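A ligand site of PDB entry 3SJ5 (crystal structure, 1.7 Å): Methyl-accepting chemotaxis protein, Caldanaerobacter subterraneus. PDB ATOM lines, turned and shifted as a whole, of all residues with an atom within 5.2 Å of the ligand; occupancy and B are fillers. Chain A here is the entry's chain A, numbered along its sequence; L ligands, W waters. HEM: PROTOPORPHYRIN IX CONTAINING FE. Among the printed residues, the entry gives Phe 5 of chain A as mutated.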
ATOM      1  N   MET A   1       2.762  -4.748 -10.511  1.00  0.00           N
ATOM      2  CA  MET A   1       1.588  -3.881 -10.517  1.00  0.00           C
ATOM      3  C   MET A   1       1.731  -2.753 -11.536  1.00  0.00           C
ATOM      4  O   MET A   1       2.839  -2.374 -11.900  1.00  0.00           O
ATOM      5  CB  MET A   1       1.338  -3.287  -9.130  1.00  0.00           C
ATOM      6  CG  MET A   1      -0.001  -2.596  -9.002  1.00  0.00           C
ATOM      7  SD  MET A   1      -1.325  -3.749  -9.387  1.00  0.00           S
ATOM      8  CE  MET A   1      -0.849  -5.094  -8.288  1.00  0.00           C
ATOM      9  N   LYS A   2       0.604  -2.216 -12.002  1.00  0.00           N
ATOM     10  CA  LYS A   2       0.628  -1.151 -12.995  1.00  0.00           C
ATOM     11  C   LYS A   2       1.030   0.183 -12.382  1.00  0.00           C
ATOM     12  O   LYS A   2       0.801   0.427 -11.202  1.00  0.00           O
ATOM     13  CB  LYS A   2      -0.724  -1.041 -13.698  1.00  0.00           C
ATOM     14  CG  LYS A   2      -1.211  -2.355 -14.272  1.00  0.00           C
ATOM     15  CD  LYS A   2      -2.561  -2.198 -14.955  1.00  0.00           C
ATOM     16  CE  LYS A   2      -3.201  -3.544 -15.219  1.00  0.00           C
ATOM     17  NZ  LYS A   2      -4.494  -3.416 -15.930  1.00  0.00           N
ATOM     18  N   PHE A   5      -1.633   3.313 -11.055  1.00  0.00           N
ATOM     19  CA  PHE A   5      -2.419   2.851  -9.914  1.00  0.00           C
ATOM     20  C   PHE A   5      -1.555   2.961  -8.675  1.00  0.00           C
ATOM     21  O   PHE A   5      -1.936   3.587  -7.710  1.00  0.00           O
ATOM     22  CB  PHE A   5      -2.890   1.412 -10.062  1.00  0.00           C
ATOM     23  CG  PHE A   5      -3.940   1.213 -11.127  1.00  0.00           C
ATOM     24  CD1 PHE A   5      -4.446  -0.044 -11.379  1.00  0.00           C
ATOM     25  CD2 PHE A   5      -4.403   2.287 -11.873  1.00  0.00           C
ATOM     26  CE1 PHE A   5      -5.415  -0.232 -12.346  1.00  0.00           C
ATOM     27  CE2 PHE A   5      -5.359   2.110 -12.853  1.00  0.00           C
ATOM     28  CZ  PHE A   5      -5.871   0.846 -13.088  1.00  0.00           C
ATOM     29  N   ILE A  75     -11.380   4.291  -3.918  1.00  0.00           N
ATOM     30  CA  ILE A  75     -12.637   4.208  -4.683  1.00  0.00           C
ATOM     31  C   ILE A  75     -12.940   5.539  -5.363  1.00  0.00           C
ATOM     32  O   ILE A  75     -13.392   5.582  -6.512  1.00  0.00           O
ATOM     33  CB  ILE A  75     -13.824   3.756  -3.799  1.00  0.00           C
ATOM     34  CG1 ILE A  75     -13.593   2.336  -3.292  1.00  0.00           C
ATOM     35  CG2 ILE A  75     -15.149   3.826  -4.578  1.00  0.00           C
ATOM     36  CD1 ILE A  75     -13.633   1.239  -4.392  1.00  0.00           C
ATOM     37  N   PHE A  78     -10.998   5.798  -8.571  1.00  0.00           N
ATOM     38  CA  PHE A  78     -11.543   4.975  -9.647  1.00  0.00           C
ATOM     39  C   PHE A  78     -12.805   5.596 -10.256  1.00  0.00           C
ATOM     40  O   PHE A  78     -13.114   5.335 -11.419  1.00  0.00           O
ATOM     41  CB  PHE A  78     -11.765   3.526  -9.192  1.00  0.00           C
ATOM     42  CG  PHE A  78     -10.510   2.684  -9.218  1.00  0.00           C
ATOM     43  CD1 PHE A  78     -10.101   2.068 -10.383  1.00  0.00           C
ATOM     44  CD2 PHE A  78      -9.744   2.525  -8.076  1.00  0.00           C
ATOM     45  CE1 PHE A  78      -8.953   1.301 -10.412  1.00  0.00           C
ATOM     46  CE2 PHE A  78      -8.583   1.754  -8.101  1.00  0.00           C
ATOM     47  CZ  PHE A  78      -8.187   1.142  -9.269  1.00  0.00           C
ATOM     48  N   PHE A  82     -13.140   5.769 -14.211  1.00  0.00           N
ATOM     49  CA  PHE A  82     -14.179   4.909 -14.769  1.00  0.00           C
ATOM     50  C   PHE A  82     -15.587   5.305 -14.277  1.00  0.00           C
ATOM     51  O   PHE A  82     -16.266   4.522 -13.620  1.00  0.00           O
ATOM     52  CB  PHE A  82     -13.884   3.433 -14.435  1.00  0.00           C
ATOM     53  CG  PHE A  82     -12.458   3.006 -14.719  1.00  0.00           C
ATOM     54  CD1 PHE A  82     -11.439   3.279 -13.814  1.00  0.00           C
ATOM     55  CD2 PHE A  82     -12.138   2.315 -15.876  1.00  0.00           C
ATOM     56  CE1 PHE A  82     -10.129   2.888 -14.064  1.00  0.00           C
ATOM     57  CE2 PHE A  82     -10.820   1.920 -16.136  1.00  0.00           C
ATOM     58  CZ  PHE A  82      -9.820   2.205 -15.232  1.00  0.00           C
ATOM     59  N   TYR A  85     -18.995   3.006 -14.370  1.00  0.00           N
ATOM     60  CA  TYR A  85     -19.245   1.920 -13.434  1.00  0.00           C
ATOM     61  C   TYR A  85     -20.074   2.404 -12.252  1.00  0.00           C
ATOM     62  O   TYR A  85     -20.752   1.621 -11.595  1.00  0.00           O
ATOM     63  CB  TYR A  85     -17.949   1.304 -12.914  1.00  0.00           C
ATOM     64  CG  TYR A  85     -17.159   0.557 -13.959  1.00  0.00           C
ATOM     65  CD1 TYR A  85     -15.775   0.623 -13.962  1.00  0.00           C
ATOM     66  CD2 TYR A  85     -17.779  -0.216 -14.925  1.00  0.00           C
ATOM     67  CE1 TYR A  85     -15.035  -0.043 -14.909  1.00  0.00           C
ATOM     68  CE2 TYR A  85     -17.041  -0.895 -15.878  1.00  0.00           C
ATOM     69  CZ  TYR A  85     -15.670  -0.803 -15.863  1.00  0.00           C
ATOM     70  OH  TYR A  85     -14.916  -1.464 -16.793  1.00  0.00           O
ATOM     71  N   PHE A  86     -20.021   3.703 -11.988  1.00  0.00           N
ATOM     72  CA  PHE A  86     -20.699   4.299 -10.848  1.00  0.00           C
ATOM     73  C   PHE A  86     -22.044   4.910 -11.205  1.00  0.00           C
ATOM     74  O   PHE A  86     -22.967   4.902 -10.403  1.00  0.00           O
ATOM     75  CB  PHE A  86     -19.810   5.369 -10.192  1.00  0.00           C
ATOM     76  CG  PHE A  86     -18.527   4.829  -9.611  1.00  0.00           C
ATOM     77  CD1 PHE A  86     -18.417   4.593  -8.243  1.00  0.00           C
ATOM     78  CD2 PHE A  86     -17.429   4.568 -10.425  1.00  0.00           C
ATOM     79  CE1 PHE A  86     -17.234   4.102  -7.695  1.00  0.00           C
ATOM     80  CE2 PHE A  86     -16.248   4.080  -9.899  1.00  0.00           C
ATOM     81  CZ  PHE A  86     -16.146   3.848  -8.521  1.00  0.00           C
ATOM     82  N   PHE A  94     -22.962  -2.605  -8.046  1.00  0.00           N
ATOM     83  CA  PHE A  94     -21.548  -2.262  -8.161  1.00  0.00           C
ATOM     84  C   PHE A  94     -20.677  -3.413  -7.657  1.00  0.00           C
ATOM     85  O   PHE A  94     -19.783  -3.887  -8.364  1.00  0.00           O
ATOM     86  CB  PHE A  94     -21.271  -0.956  -7.407  1.00  0.00           C
ATOM     87  CG  PHE A  94     -19.831  -0.492  -7.486  1.00  0.00           C
ATOM     88  CD1 PHE A  94     -19.363   0.201  -8.596  1.00  0.00           C
ATOM     89  CD2 PHE A  94     -18.966  -0.726  -6.423  1.00  0.00           C
ATOM     90  CE1 PHE A  94     -18.041   0.639  -8.643  1.00  0.00           C
ATOM     91  CE2 PHE A  94     -17.655  -0.296  -6.466  1.00  0.00           C
ATOM     92  CZ  PHE A  94     -17.194   0.392  -7.580  1.00  0.00           C
ATOM     93  N   LEU A  95     -20.952  -3.896  -6.445  1.00  0.00           N
ATOM     94  CA  LEU A  95     -20.137  -4.972  -5.894  1.00  0.00           C
ATOM     95  C   LEU A  95     -20.277  -6.257  -6.709  1.00  0.00           C
ATOM     96  O   LEU A  95     -19.298  -6.940  -6.936  1.00  0.00           O
ATOM     97  CB  LEU A  95     -20.475  -5.217  -4.422  1.00  0.00           C
ATOM     98  CG  LEU A  95     -20.147  -4.045  -3.506  1.00  0.00           C
ATOM     99  CD1 LEU A  95     -20.683  -4.343  -2.084  1.00  0.00           C
ATOM    100  CD2 LEU A  95     -18.651  -3.826  -3.455  1.00  0.00           C
ATOM    101  N   MET A  98     -17.960  -6.487  -9.812  1.00  0.00           N
ATOM    102  CA  MET A  98     -16.521  -6.277  -9.670  1.00  0.00           C
ATOM    103  C   MET A  98     -15.681  -7.419 -10.232  1.00  0.00           C
ATOM    104  O   MET A  98     -14.639  -7.184 -10.835  1.00  0.00           O
ATOM    105  CB  MET A  98     -16.139  -6.015  -8.202  1.00  0.00           C
ATOM    106  CG  MET A  98     -16.474  -4.614  -7.690  1.00  0.00           C
ATOM    107  SD  MET A  98     -15.621  -3.316  -8.597  1.00  0.00           S
ATOM    108  CE  MET A  98     -16.894  -2.713  -9.702  1.00  0.00           C
ATOM    109  N   VAL A 101     -15.469  -6.884 -13.934  1.00  0.00           N
ATOM    110  CA  VAL A 101     -14.728  -5.664 -14.232  1.00  0.00           C
ATOM    111  C   VAL A 101     -13.234  -5.930 -14.158  1.00  0.00           C
ATOM    112  O   VAL A 101     -12.470  -5.503 -15.016  1.00  0.00           O
ATOM    113  CB  VAL A 101     -15.120  -4.511 -13.289  1.00  0.00           C
ATOM    114  CG1 VAL A 101     -14.059  -3.395 -13.316  1.00  0.00           C
ATOM    115  CG2 VAL A 101     -16.508  -3.979 -13.647  1.00  0.00           C
ATOM    116  N   HIS A 102     -12.814  -6.693 -13.150  1.00  0.00           N
ATOM    117  CA  HIS A 102     -11.384  -6.976 -13.035  1.00  0.00           C
ATOM    118  C   HIS A 102     -10.853  -7.916 -14.128  1.00  0.00           C
ATOM    119  O   HIS A 102      -9.697  -7.812 -14.547  1.00  0.00           O
ATOM    120  CB  HIS A 102     -11.035  -7.453 -11.614  1.00  0.00           C
ATOM    121  CG  HIS A 102     -11.143  -6.371 -10.578  1.00  0.00           C
ATOM    122  ND1 HIS A 102     -12.361  -5.835 -10.183  1.00  0.00           N
ATOM    123  CD2 HIS A 102     -10.193  -5.710  -9.883  1.00  0.00           C
ATOM    124  CE1 HIS A 102     -12.147  -4.884  -9.292  1.00  0.00           C
ATOM    125  NE2 HIS A 102     -10.846  -4.805  -9.090  1.00  0.00           N
ATOM    126  N   LEU A 105     -10.882  -5.614 -17.474  1.00  0.00           N
ATOM    127  CA  LEU A 105      -9.851  -4.574 -17.532  1.00  0.00           C
ATOM    128  C   LEU A 105      -8.423  -5.103 -17.666  1.00  0.00           C
ATOM    129  O   LEU A 105      -7.496  -4.326 -17.933  1.00  0.00           O
ATOM    130  CB  LEU A 105      -9.954  -3.622 -16.322  1.00  0.00           C
ATOM    131  CG  LEU A 105     -11.171  -2.702 -16.308  1.00  0.00           C
ATOM    132  CD1 LEU A 105     -11.134  -1.802 -15.088  1.00  0.00           C
ATOM    133  CD2 LEU A 105     -11.247  -1.867 -17.597  1.00  0.00           C
ATOM    134  N   THR A 106      -8.223  -6.405 -17.481  1.00  0.00           N
ATOM    135  CA  THR A 106      -6.894  -6.987 -17.567  1.00  0.00           C
ATOM    136  C   THR A 106      -6.713  -8.012 -18.703  1.00  0.00           C
ATOM    137  O   THR A 106      -5.618  -8.508 -18.917  1.00  0.00           O
ATOM    138  CB  THR A 106      -6.493  -7.659 -16.222  1.00  0.00           C
ATOM    139  OG1 THR A 106      -7.395  -8.733 -15.925  1.00  0.00           O
ATOM    140  CG2 THR A 106      -6.514  -6.638 -15.072  1.00  0.00           C
ATOM    141  N   THR A 113      -2.988 -11.427 -13.889  1.00  0.00           N
ATOM    142  CA  THR A 113      -3.511 -12.238 -12.811  1.00  0.00           C
ATOM    143  C   THR A 113      -4.369 -11.363 -11.892  1.00  0.00           C
ATOM    144  O   THR A 113      -3.962 -11.025 -10.780  1.00  0.00           O
ATOM    145  CB  THR A 113      -2.392 -12.891 -11.978  1.00  0.00           C
ATOM    146  OG1 THR A 113      -1.433 -11.887 -11.611  1.00  0.00           O
ATOM    147  CG2 THR A 113      -1.698 -13.975 -12.776  1.00  0.00           C
ATOM    148  N   PRO A 114      -5.556 -10.951 -12.373  1.00  0.00           N
ATOM    149  CA  PRO A 114      -6.374 -10.072 -11.531  1.00  0.00           C
ATOM    150  C   PRO A 114      -6.900 -10.838 -10.311  1.00  0.00           C
ATOM    151  O   PRO A 114      -7.002 -12.054 -10.364  1.00  0.00           O
ATOM    152  CB  PRO A 114      -7.549  -9.711 -12.446  1.00  0.00           C
ATOM    153  CG  PRO A 114      -7.621 -10.861 -13.454  1.00  0.00           C
ATOM    154  CD  PRO A 114      -6.176 -11.251 -13.672  1.00  0.00           C
ATOM    155  N   PRO A 115      -7.251 -10.112  -9.251  1.00  0.00           N
ATOM    156  CA  PRO A 115      -7.949 -10.812  -8.159  1.00  0.00           C
ATOM    157  C   PRO A 115      -9.311 -11.304  -8.654  1.00  0.00           C
ATOM    158  O   PRO A 115      -9.953 -10.674  -9.517  1.00  0.00           O
ATOM    159  CB  PRO A 115      -8.151  -9.704  -7.142  1.00  0.00           C
ATOM    160  CG  PRO A 115      -8.314  -8.468  -7.975  1.00  0.00           C
ATOM    161  CD  PRO A 115      -7.339  -8.651  -9.110  1.00  0.00           C
ATOM    162  N   LEU A 117     -13.189 -11.850  -7.454  1.00  0.00           N
ATOM    163  CA  LEU A 117     -14.035 -11.149  -6.491  1.00  0.00           C
ATOM    164  C   LEU A 117     -15.489 -11.627  -6.580  1.00  0.00           C
ATOM    165  O   LEU A 117     -16.438 -10.840  -6.515  1.00  0.00           O
ATOM    166  CB  LEU A 117     -13.956  -9.631  -6.737  1.00  0.00           C
ATOM    167  CG  LEU A 117     -12.549  -9.030  -6.690  1.00  0.00           C
ATOM    168  CD1 LEU A 117     -12.529  -7.639  -7.300  1.00  0.00           C
ATOM    169  CD2 LEU A 117     -12.015  -8.981  -5.229  1.00  0.00           C
ATOM    170  N   MET A 129     -18.990 -12.407  -0.603  1.00  0.00           N
ATOM    171  CA  MET A 129     -18.035 -12.055  -1.658  1.00  0.00           C
ATOM    172  C   MET A 129     -16.703 -12.639  -1.237  1.00  0.00           C
ATOM    173  O   MET A 129     -16.324 -12.543  -0.053  1.00  0.00           O
ATOM    174  CB  MET A 129     -17.942 -10.538  -1.787  1.00  0.00           C
ATOM    175  CG  MET A 129     -17.040 -10.079  -2.881  1.00  0.00           C
ATOM    176  SD  MET A 129     -17.104  -8.280  -2.998  1.00  0.00           S
ATOM    177  CE  MET A 129     -16.438  -7.994  -4.644  1.00  0.00           C
ATOM    178  N   TYR A 131     -12.587 -12.799  -1.969  1.00  0.00           N
ATOM    179  CA  TYR A 131     -11.324 -12.341  -2.556  1.00  0.00           C
ATOM    180  C   TYR A 131     -10.428 -13.541  -2.764  1.00  0.00           C
ATOM    181  O   TYR A 131     -10.219 -14.322  -1.840  1.00  0.00           O
ATOM    182  CB  TYR A 131     -10.669 -11.350  -1.579  1.00  0.00           C
ATOM    183  CG  TYR A 131      -9.240 -10.986  -1.928  1.00  0.00           C
ATOM    184  CD1 TYR A 131      -8.953 -10.122  -2.979  1.00  0.00           C
ATOM    185  CD2 TYR A 131      -8.176 -11.498  -1.189  1.00  0.00           C
ATOM    186  CE1 TYR A 131      -7.629  -9.779  -3.279  1.00  0.00           C
ATOM    187  CE2 TYR A 131      -6.852 -11.146  -1.475  1.00  0.00           C
ATOM    188  CZ  TYR A 131      -6.584 -10.295  -2.525  1.00  0.00           C
ATOM    189  OH  TYR A 131      -5.268  -9.963  -2.799  1.00  0.00           O
ATOM    190  N   SER A 133      -6.616 -14.327  -4.539  1.00  0.00           N
ATOM    191  CA  SER A 133      -5.452 -13.759  -5.224  1.00  0.00           C
ATOM    192  C   SER A 133      -4.154 -14.298  -4.649  1.00  0.00           C
ATOM    193  O   SER A 133      -4.086 -14.611  -3.473  1.00  0.00           O
ATOM    194  CB  SER A 133      -5.451 -12.222  -5.092  1.00  0.00           C
ATOM    195  OG  SER A 133      -4.368 -11.641  -5.808  1.00  0.00           O
ATOM    196  N   ARG A 135      -1.720 -12.291  -4.294  1.00  0.00           N
ATOM    197  CA  ARG A 135      -1.099 -11.077  -3.742  1.00  0.00           C
ATOM    198  C   ARG A 135      -1.349 -10.812  -2.245  1.00  0.00           C
ATOM    199  O   ARG A 135      -0.647  -9.999  -1.631  1.00  0.00           O
ATOM    200  CB  ARG A 135      -1.540  -9.863  -4.558  1.00  0.00           C
ATOM    201  CG  ARG A 135      -0.942  -9.820  -5.966  1.00  0.00           C
ATOM    202  CD  ARG A 135      -1.191  -8.455  -6.569  1.00  0.00           C
ATOM    203  NE  ARG A 135      -0.758  -8.346  -7.955  1.00  0.00           N
ATOM    204  CZ  ARG A 135      -1.550  -8.494  -9.008  1.00  0.00           C
ATOM    205  NH1 ARG A 135      -2.849  -8.767  -8.850  1.00  0.00           N
ATOM    206  NH2 ARG A 135      -1.043  -8.379 -10.233  1.00  0.00           N
ATOM    207  N   MET A 137      -3.674  -9.222  -0.551  1.00  0.00           N
ATOM    208  CA  MET A 137      -3.984  -7.845  -0.198  1.00  0.00           C
ATOM    209  C   MET A 137      -5.312  -7.755   0.562  1.00  0.00           C
ATOM    210  O   MET A 137      -6.254  -7.076   0.145  1.00  0.00           O
ATOM    211  CB  MET A 137      -3.958  -6.961  -1.446  1.00  0.00           C
ATOM    212  CG  MET A 137      -2.644  -7.124  -2.197  1.00  0.00           C
ATOM    213  SD  MET A 137      -2.480  -5.970  -3.582  1.00  0.00           S
ATOM    214  CE  MET A 137      -2.255  -4.437  -2.671  1.00  0.00           C
ATOM    215  N   TYR A 140      -6.443  -4.147   1.812  1.00  0.00           N
ATOM    216  CA  TYR A 140      -6.828  -3.320   0.672  1.00  0.00           C
ATOM    217  C   TYR A 140      -8.241  -3.715   0.190  1.00  0.00           C
ATOM    218  O   TYR A 140      -9.100  -2.853  -0.057  1.00  0.00           O
ATOM    219  CB  TYR A 140      -5.794  -3.508  -0.425  1.00  0.00           C
ATOM    220  CG  TYR A 140      -5.975  -2.624  -1.647  1.00  0.00           C
ATOM    221  CD1 TYR A 140      -6.002  -1.237  -1.540  1.00  0.00           C
ATOM    222  CD2 TYR A 140      -6.073  -3.200  -2.909  1.00  0.00           C
ATOM    223  CE1 TYR A 140      -6.150  -0.437  -2.663  1.00  0.00           C
ATOM    224  CE2 TYR A 140      -6.216  -2.408  -4.033  1.00  0.00           C
ATOM    225  CZ  TYR A 140      -6.238  -1.035  -3.897  1.00  0.00           C
ATOM    226  OH  TYR A 140      -6.399  -0.265  -5.036  1.00  0.00           O
ATOM    227  N   PHE A 141      -8.473  -5.019   0.071  1.00  0.00           N
ATOM    228  CA  PHE A 141      -9.784  -5.528  -0.290  1.00  0.00           C
ATOM    229  C   PHE A 141     -10.884  -5.025   0.669  1.00  0.00           C
ATOM    230  O   PHE A 141     -11.905  -4.459   0.236  1.00  0.00           O
ATOM    231  CB  PHE A 141      -9.715  -7.070  -0.335  1.00  0.00           C
ATOM    232  CG  PHE A 141     -11.070  -7.762  -0.426  1.00  0.00           C
ATOM    233  CD1 PHE A 141     -11.770  -7.817  -1.626  1.00  0.00           C
ATOM    234  CD2 PHE A 141     -11.604  -8.391   0.690  1.00  0.00           C
ATOM    235  CE1 PHE A 141     -12.995  -8.484  -1.699  1.00  0.00           C
ATOM    236  CE2 PHE A 141     -12.822  -9.045   0.635  1.00  0.00           C
ATOM    237  CZ  PHE A 141     -13.525  -9.104  -0.556  1.00  0.00           C
ATOM    238  N   LEU A 144     -11.485  -1.232   0.301  1.00  0.00           N
ATOM    239  CA  LEU A 144     -12.216  -0.897  -0.927  1.00  0.00           C
ATOM    240  C   LEU A 144     -13.713  -1.118  -0.719  1.00  0.00           C
ATOM    241  O   LEU A 144     -14.533  -0.323  -1.175  1.00  0.00           O
ATOM    242  CB  LEU A 144     -11.716  -1.731  -2.098  1.00  0.00           C
ATOM    243  CG  LEU A 144     -10.349  -1.313  -2.625  1.00  0.00           C
ATOM    244  CD1 LEU A 144      -9.738  -2.427  -3.495  1.00  0.00           C
ATOM    245  CD2 LEU A 144     -10.470   0.005  -3.411  1.00  0.00           C
ATOM    246  N   ILE A 145     -14.076  -2.177   0.001  1.00  0.00           N
ATOM    247  CA  ILE A 145     -15.491  -2.387   0.305  1.00  0.00           C
ATOM    248  C   ILE A 145     -16.057  -1.236   1.149  1.00  0.00           C
ATOM    249  O   ILE A 145     -17.129  -0.712   0.874  1.00  0.00           O
ATOM    250  CB  ILE A 145     -15.715  -3.750   0.999  1.00  0.00           C
ATOM    251  CG1 ILE A 145     -15.443  -4.888   0.002  1.00  0.00           C
ATOM    252  CG2 ILE A 145     -17.157  -3.839   1.526  1.00  0.00           C
ATOM    253  CD1 ILE A 145     -15.381  -6.249   0.684  1.00  0.00           C
ATOM    254  N   SER A 148     -16.435   1.872  -0.855  1.00  0.00           N
ATOM    255  CA  SER A 148     -17.599   1.809  -1.763  1.00  0.00           C
ATOM    256  C   SER A 148     -18.865   2.177  -1.013  1.00  0.00           C
ATOM    257  O   SER A 148     -19.720   2.911  -1.528  1.00  0.00           O
ATOM    258  CB  SER A 148     -17.724   0.426  -2.411  1.00  0.00           C
ATOM    259  OG  SER A 148     -16.580   0.139  -3.188  1.00  0.00           O
HETATM  260  CHA HEM L   1      -6.665  -4.359  -8.276  1.00  0.00           C
HETATM  261  CHB HEM L   1      -9.851  -2.105 -11.162  1.00  0.00           C
HETATM  262  CHC HEM L   1     -12.787  -1.564  -7.379  1.00  0.00           C
HETATM  263  CHD HEM L   1     -10.434  -5.289  -5.342  1.00  0.00           C
HETATM  264  C1A HEM L   1      -7.270  -3.811  -9.398  1.00  0.00           C
HETATM  265  C2A HEM L   1      -6.726  -3.782 -10.738  1.00  0.00           C
HETATM  266  C3A HEM L   1      -7.602  -3.166 -11.533  1.00  0.00           C
HETATM  267  C4A HEM L   1      -8.747  -2.775 -10.724  1.00  0.00           C
HETATM  268  CMA HEM L   1      -7.448  -2.915 -13.048  1.00  0.00           C
HETATM  269  CAA HEM L   1      -5.362  -4.381 -11.170  1.00  0.00           C
HETATM  270  CBA HEM L   1      -5.461  -5.894 -11.266  1.00  0.00           C
HETATM  271  CGA HEM L   1      -4.167  -6.456 -11.750  1.00  0.00           C
HETATM  272  O1A HEM L   1      -4.036  -7.702 -11.776  1.00  0.00           O
HETATM  273  O2A HEM L   1      -3.253  -5.668 -12.118  1.00  0.00           O
HETATM  274  C1B HEM L   1     -10.866  -1.658 -10.369  1.00  0.00           C
HETATM  275  C2B HEM L   1     -11.890  -0.701 -10.741  1.00  0.00           C
HETATM  276  C3B HEM L   1     -12.705  -0.538  -9.688  1.00  0.00           C
HETATM  277  C4B HEM L   1     -12.209  -1.395  -8.627  1.00  0.00           C
HETATM  278  CMB HEM L   1     -11.995   0.031 -12.104  1.00  0.00           C
HETATM  279  CAB HEM L   1     -13.945   0.363  -9.542  1.00  0.00           C
HETATM  280  CBB HEM L   1     -14.501   1.000 -10.567  1.00  0.00           C
HETATM  281  C1C HEM L   1     -12.486  -2.630  -6.556  1.00  0.00           C
HETATM  282  C2C HEM L   1     -13.314  -3.158  -5.478  1.00  0.00           C
HETATM  283  C3C HEM L   1     -12.642  -4.184  -4.929  1.00  0.00           C
HETATM  284  C4C HEM L   1     -11.406  -4.350  -5.627  1.00  0.00           C
HETATM  285  CMC HEM L   1     -14.690  -2.613  -5.061  1.00  0.00           C
HETATM  286  CAC HEM L   1     -13.087  -5.116  -3.776  1.00  0.00           C
HETATM  287  CBC HEM L   1     -14.377  -5.232  -3.449  1.00  0.00           C
HETATM  288  C1D HEM L   1      -9.140  -5.229  -5.803  1.00  0.00           C
HETATM  289  C2D HEM L   1      -7.974  -5.709  -5.120  1.00  0.00           C
HETATM  290  C3D HEM L   1      -6.784  -5.434  -6.033  1.00  0.00           C
HETATM  291  C4D HEM L   1      -7.351  -4.792  -7.182  1.00  0.00           C
HETATM  292  CMD HEM L   1      -7.919  -6.392  -3.742  1.00  0.00           C
HETATM  293  CAD HEM L   1      -5.310  -5.738  -5.721  1.00  0.00           C
HETATM  294  CBD HEM L   1      -4.800  -6.840  -6.629  1.00  0.00           C
HETATM  295  CGD HEM L   1      -4.879  -8.153  -5.881  1.00  0.00           C
HETATM  296  O1D HEM L   1      -5.204  -8.178  -4.663  1.00  0.00           O
HETATM  297  O2D HEM L   1      -4.609  -9.187  -6.542  1.00  0.00           O
HETATM  298  NA  HEM L   1      -8.499  -3.187  -9.421  1.00  0.00           N
HETATM  299  NB  HEM L   1     -11.102  -2.070  -9.070  1.00  0.00           N
HETATM  300  NC  HEM L   1     -11.338  -3.391  -6.615  1.00  0.00           N
HETATM  301  ND  HEM L   1      -8.740  -4.674  -7.014  1.00  0.00           N
HETATM  302 FE   HEM L   1      -9.937  -3.321  -8.043  1.00  0.00          FE
HETATM  303  O   HOH W   1      -8.939  -1.716  -6.985  1.00  0.00           O
HETATM  304  O   HOH W   2      -3.741 -11.844  -8.402  1.00  0.00           O
HETATM  305  O   HOH W   3      -2.046  -8.839 -13.082  1.00  0.00           O
HETATM  306  O   HOH W   4      -0.471  -6.700 -12.952  1.00  0.00           O
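An iron atom (FE) of the ligand is bound by a ring nitrogen (NE2) of His 102 (2.0 Å).
The side-chain hydroxyl (OG) of Ser 133 sits at hydrogen-bond distance from an oxygen (O2D) of the ligand, at 2.6 Å.
O1D of the ligand is in hydrogen-bond range of OH of Tyr 131, 2.6 Å away.
O2D of the ligand lies within salt-bridge range of NH1 of Arg 135 (2.9 Å).
ND1 of His 102 lies within hydrogen-bond range of O of Met 98 (2.7 Å).
O of His 102 lies within hydrogen-bond range of OG1 of Thr 106.
OG of Ser 133 is in hydrogen-bond range of N of Arg 135.
OH of Tyr 131 is in hydrogen-bond range of N of Met 137 (2.9 Å).
The guanidinium group (NH1) of Arg 135 sits at hydrogen-bond distance from the backbone carbonyl oxygen (O) of Thr 113 (3.2 Å).
O of Leu 144 lies within hydrogen-bond range of OG of Ser 148 (2.9 Å).
An oxygen (O1A) of the ligand sits close to the backbone carbonyl oxygen of Thr 113, 3.5 Å away.
An oxygen (O1D) of the ligand sits close to the side-chain sulfur (SD) of Met 137, 3.7 Å away.
SD of Met 1 touches O2A of the ligand, at 3.9 Å.
CE of Lys 2 touches O2A of the ligand, at 3.8 Å.
CE1 of Phe 5 touches CMA of the ligand, 3.4 Å away.
CD1 of Phe 78 touches CMB of the ligand (3.3 Å).
Phe 82 touches the ligand (CD1 to CMB, 3.7 Å).
CD1 of Tyr 85 touches CBB of the ligand (3.6 Å).
Phe 86 touches the ligand (CE2 to CBB, 3.6 Å).
Phe 94 touches the ligand.
SD of Met 98 touches CHC of the ligand (3.5 Å).
Leu 105 touches the ligand (CD1 to CMB, 3.6 Å).
Pro 114 touches the ligand (CA to O1A, 3.3 Å).
Pro 115 touches the ligand (CB to O2D, 3.6 Å).
CD1 of Leu 117 touches CHD of the ligand, 3.7 Å away.
Met 129 touches the ligand (CE to CBC, 3.6 Å).
Tyr 140 touches the ligand.
Phe 141 touches the ligand (CD1 to CAC, 3.7 Å).
Leu 144 touches the ligand (CD1 to C4C, 3.3 Å).
Ile 145 touches the ligand (CG1 to CBC, 3.6 Å).
OG of Ser 148 touches CMC of the ligand (3.8 Å).
Within 4 Å of the ligand: Met 1, Lys 2, Phe 5, Phe 78, Phe 82, Tyr 85, Phe 86, Phe 94, Met 98, His 102, Leu 105, Thr 113, Pro 114, Pro 115, Leu 117, Met 129, Tyr 131, Ser 133, Arg 135, Met 137, Tyr 140, Phe 141, Leu 144, Ile 145 and Ser 148.
The nearest printed residue that does not touch the ligand is Thr 106 (4.02 Å).
Water W3 lies within hydrogen-bond range of O1A of the ligand, N of Thr 113 and NH2 of Arg 135.
Water W4 bridges an oxygen (O2A) of the ligand and the guanidinium group of Arg 135.
Water W2 lies within hydrogen-bond range of O of Thr 113 (2.5 Å), OG of Ser 133 (2.7 Å), NH1 of Arg 135 (3.2 Å) and O2D of the ligand (3.4 Å).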
